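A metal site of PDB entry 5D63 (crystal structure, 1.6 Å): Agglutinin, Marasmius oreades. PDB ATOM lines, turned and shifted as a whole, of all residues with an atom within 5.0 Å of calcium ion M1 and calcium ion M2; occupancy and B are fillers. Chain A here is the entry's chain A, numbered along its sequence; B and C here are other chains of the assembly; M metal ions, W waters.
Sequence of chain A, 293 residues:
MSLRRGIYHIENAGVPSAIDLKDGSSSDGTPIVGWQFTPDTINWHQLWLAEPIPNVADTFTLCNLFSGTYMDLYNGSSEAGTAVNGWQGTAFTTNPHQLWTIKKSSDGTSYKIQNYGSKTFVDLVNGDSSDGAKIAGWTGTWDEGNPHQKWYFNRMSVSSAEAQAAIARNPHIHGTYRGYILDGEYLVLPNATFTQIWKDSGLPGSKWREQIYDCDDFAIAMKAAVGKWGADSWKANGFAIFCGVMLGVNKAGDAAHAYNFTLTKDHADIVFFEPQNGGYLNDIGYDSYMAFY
Within 4 Å of calcium ion M1: Gln 211, Asp 214, Asp 216, Asp 217 and Asp 183 of chain B. The nearest printed residue that does not touch calcium ion M1 is Ala 240 of chain B (4.4 Å).
Five residues have an atom within 4 Å of calcium ion M2: Asp 214, Asp 216, Leu 182 of chain B, Asp 183 of chain B and Ala 3 of chain C. Along chain A the residues within 4 Å of calcium ion M2 span positions 214 to 216. The nearest printed residue that does not touch calcium ion M2 is Asp 4 of chain C (4.03 Å).
Calcium ion M1 is bound by OD1 of Asp 214, O of Gln 211, OD2 of Asp 217, water W1, OD2 of Asp 216, OD2 of Asp 183 of chain B and OD1 of Asp 183 of chain B.
Calcium ion M2 is bound by O of Leu 182 of chain B (2.3 Å), OD1 of Asp 183 of chain B (2.3 Å), OD2 of Asp 214 (2.3 Å), OD1 of Asp 216 (2.3 Å), O of Ala 3 of chain C (2.3 Å) and water W2 (2.5 Å). Calcium ion M2 has six donor atoms within binding distance.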
ATOM      1  N   GLN A 211      25.013 -16.027  -1.939  1.00  0.00           N
ATOM      2  CA  GLN A 211      26.166 -16.508  -1.170  1.00  0.00           C
ATOM      3  C   GLN A 211      26.922 -17.741  -1.717  1.00  0.00           C
ATOM      4  O   GLN A 211      28.148 -17.759  -1.702  1.00  0.00           O
ATOM      5  CB  GLN A 211      25.834 -16.744   0.296  1.00  0.00           C
ATOM      6  CG  GLN A 211      25.418 -15.426   1.053  1.00  0.00           C
ATOM      7  CD  GLN A 211      25.461 -15.590   2.545  1.00  0.00           C
ATOM      8  OE1 GLN A 211      26.454 -16.037   3.119  1.00  0.00           O
ATOM      9  NE2 GLN A 211      24.380 -15.160   3.193  1.00  0.00           N
ATOM     10  N   ILE A 212      26.195 -18.756  -2.166  1.00  0.00           N
ATOM     11  CA  ILE A 212      26.821 -20.057  -2.559  1.00  0.00           C
ATOM     12  C   ILE A 212      27.512 -19.993  -3.921  1.00  0.00           C
ATOM     13  O   ILE A 212      28.438 -20.757  -4.183  1.00  0.00           O
ATOM     14  CB  ILE A 212      25.735 -21.159  -2.487  1.00  0.00           C
ATOM     15  CG1 ILE A 212      26.301 -22.583  -2.538  1.00  0.00           C
ATOM     16  CG2 ILE A 212      24.638 -20.954  -3.520  1.00  0.00           C
ATOM     17  CD1 ILE A 212      27.130 -22.970  -1.335  1.00  0.00           C
ATOM     18  N   TYR A 213      27.059 -19.130  -4.803  1.00  0.00           N
ATOM     19  CA  TYR A 213      27.843 -18.846  -6.031  1.00  0.00           C
ATOM     20  C   TYR A 213      27.541 -17.435  -6.555  1.00  0.00           C
ATOM     21  O   TYR A 213      26.780 -17.209  -7.497  1.00  0.00           O
ATOM     22  CB  TYR A 213      27.676 -19.960  -7.078  1.00  0.00           C
ATOM     23  CG  TYR A 213      28.954 -20.197  -7.816  1.00  0.00           C
ATOM     24  CD1 TYR A 213      29.972 -20.977  -7.214  1.00  0.00           C
ATOM     25  CD2 TYR A 213      29.149 -19.673  -9.106  1.00  0.00           C
ATOM     26  CE1 TYR A 213      31.131 -21.168  -7.886  1.00  0.00           C
ATOM     27  CE2 TYR A 213      30.325 -19.837  -9.752  1.00  0.00           C
ATOM     28  CZ  TYR A 213      31.293 -20.626  -9.188  1.00  0.00           C
ATOM     29  OH  TYR A 213      32.543 -20.845  -9.855  1.00  0.00           O
ATOM     30  N   ASP A 214      28.017 -16.496  -5.760  1.00  0.00           N
ATOM     31  CA  ASP A 214      27.725 -15.077  -6.006  1.00  0.00           C
ATOM     32  C   ASP A 214      28.997 -14.384  -6.503  1.00  0.00           C
ATOM     33  O   ASP A 214      29.952 -15.062  -6.977  1.00  0.00           O
ATOM     34  CB  ASP A 214      27.058 -14.388  -4.775  1.00  0.00           C
ATOM     35  CG  ASP A 214      27.976 -14.283  -3.581  1.00  0.00           C
ATOM     36  OD1 ASP A 214      28.887 -15.135  -3.410  1.00  0.00           O
ATOM     37  OD2 ASP A 214      27.739 -13.417  -2.707  1.00  0.00           O
ATOM     38  N   ASP A 216      31.758 -12.971  -5.516  1.00  0.00           N
ATOM     39  CA  ASP A 216      33.070 -13.386  -5.082  1.00  0.00           C
ATOM     40  C   ASP A 216      33.482 -14.728  -5.668  1.00  0.00           C
ATOM     41  O   ASP A 216      34.675 -14.937  -6.036  1.00  0.00           O
ATOM     42  CB  ASP A 216      33.220 -13.404  -3.568  1.00  0.00           C
ATOM     43  CG  ASP A 216      32.013 -14.007  -2.856  1.00  0.00           C
ATOM     44  OD1 ASP A 216      31.046 -13.241  -2.581  1.00  0.00           O
ATOM     45  OD2 ASP A 216      32.117 -15.220  -2.579  1.00  0.00           O
ATOM     46  N   ASP A 217      32.504 -15.652  -5.755  1.00  0.00           N
ATOM     47  CA  ASP A 217      32.825 -16.950  -6.352  1.00  0.00           C
ATOM     48  C   ASP A 217      33.209 -16.841  -7.854  1.00  0.00           C
ATOM     49  O   ASP A 217      34.172 -17.488  -8.304  1.00  0.00           O
ATOM     50  CB  ASP A 217      31.645 -17.902  -6.191  1.00  0.00           C
ATOM     51  CG  ASP A 217      31.342 -18.142  -4.748  1.00  0.00           C
ATOM     52  OD1 ASP A 217      32.089 -18.921  -4.154  1.00  0.00           O
ATOM     53  OD2 ASP A 217      30.436 -17.497  -4.195  1.00  0.00           O
ATOM     54  N   LEU B 182      33.743 -12.215   2.655  1.00  0.00           N
ATOM     55  CA  LEU B 182      33.082 -12.281   1.402  1.00  0.00           C
ATOM     56  C   LEU B 182      31.582 -12.689   1.442  1.00  0.00           C
ATOM     57  O   LEU B 182      30.821 -12.398   0.497  1.00  0.00           O
ATOM     58  CB  LEU B 182      33.837 -13.295   0.526  1.00  0.00           C
ATOM     59  CG  LEU B 182      35.329 -13.028   0.268  1.00  0.00           C
ATOM     60  CD1 LEU B 182      35.999 -14.192  -0.497  1.00  0.00           C
ATOM     61  CD2 LEU B 182      35.564 -11.838  -0.511  1.00  0.00           C
ATOM     62  N   ASP B 183      31.138 -13.422   2.485  1.00  0.00           N
ATOM     63  CA  ASP B 183      29.792 -13.909   2.610  1.00  0.00           C
ATOM     64  C   ASP B 183      29.355 -13.791   4.100  1.00  0.00           C
ATOM     65  O   ASP B 183      30.028 -13.095   4.877  1.00  0.00           O
ATOM     66  CB  ASP B 183      29.794 -15.393   2.121  1.00  0.00           C
ATOM     67  CG  ASP B 183      30.012 -15.530   0.581  1.00  0.00           C
ATOM     68  OD1 ASP B 183      29.272 -14.915  -0.207  1.00  0.00           O
ATOM     69  OD2 ASP B 183      30.949 -16.363   0.288  1.00  0.00           O
ATOM     70  N   ALA B 240      27.386 -20.003   2.279  1.00  0.00           N
ATOM     71  CA  ALA B 240      28.570 -20.385   1.582  1.00  0.00           C
ATOM     72  C   ALA B 240      29.293 -21.521   2.305  1.00  0.00           C
ATOM     73  O   ALA B 240      28.841 -21.976   3.354  1.00  0.00           O
ATOM     74  CB  ALA B 240      29.483 -19.197   1.456  1.00  0.00           C
ATOM     75  N   VAL C   2      30.294  -6.127   2.376  1.00  0.00           N
ATOM     76  CA  VAL C   2      30.602  -7.516   1.906  1.00  0.00           C
ATOM     77  C   VAL C   2      29.947  -7.799   0.549  1.00  0.00           C
ATOM     78  O   VAL C   2      28.770  -7.511   0.307  1.00  0.00           O
ATOM     79  CB  VAL C   2      30.458  -8.675   3.005  1.00  0.00           C
ATOM     80  CG1 VAL C   2      30.114  -8.176   4.411  1.00  0.00           C
ATOM     81  CG2 VAL C   2      29.592  -9.840   2.551  1.00  0.00           C
ATOM     82  N   ALA C   3      30.777  -8.340  -0.357  1.00  0.00           N
ATOM     83  CA  ALA C   3      30.414  -8.381  -1.767  1.00  0.00           C
ATOM     84  C   ALA C   3      29.331  -9.406  -2.075  1.00  0.00           C
ATOM     85  O   ALA C   3      29.428 -10.553  -1.713  1.00  0.00           O
ATOM     86  CB  ALA C   3      31.680  -8.635  -2.563  1.00  0.00           C
ATOM     87  N   ASP C   4      28.267  -9.005  -2.750  1.00  0.00           N
ATOM     88  CA  ASP C   4      27.359 -10.037  -3.316  1.00  0.00           C
ATOM     89  C   ASP C   4      27.327 -10.029  -4.809  1.00  0.00           C
ATOM     90  O   ASP C   4      26.920 -11.048  -5.418  1.00  0.00           O
ATOM     91  CB  ASP C   4      25.962  -9.895  -2.751  1.00  0.00           C
ATOM     92  CG  ASP C   4      25.303  -8.549  -3.112  1.00  0.00           C
ATOM     93  OD1 ASP C   4      25.791  -7.823  -4.024  1.00  0.00           O
ATOM     94  OD2 ASP C   4      24.283  -8.244  -2.455  1.00  0.00           O
HETATM   95 CA    CA M   1      30.152 -16.538  -2.022  1.00  0.00          CA
HETATM   96 CA    CA M   2      29.304 -12.795  -1.119  1.00  0.00          CA
HETATM   97  O   HOH W   1      31.545 -18.449  -1.593  1.00  0.00           O
HETATM   98  O   HOH W   2      27.484 -12.061   0.361  1.00  0.00           O
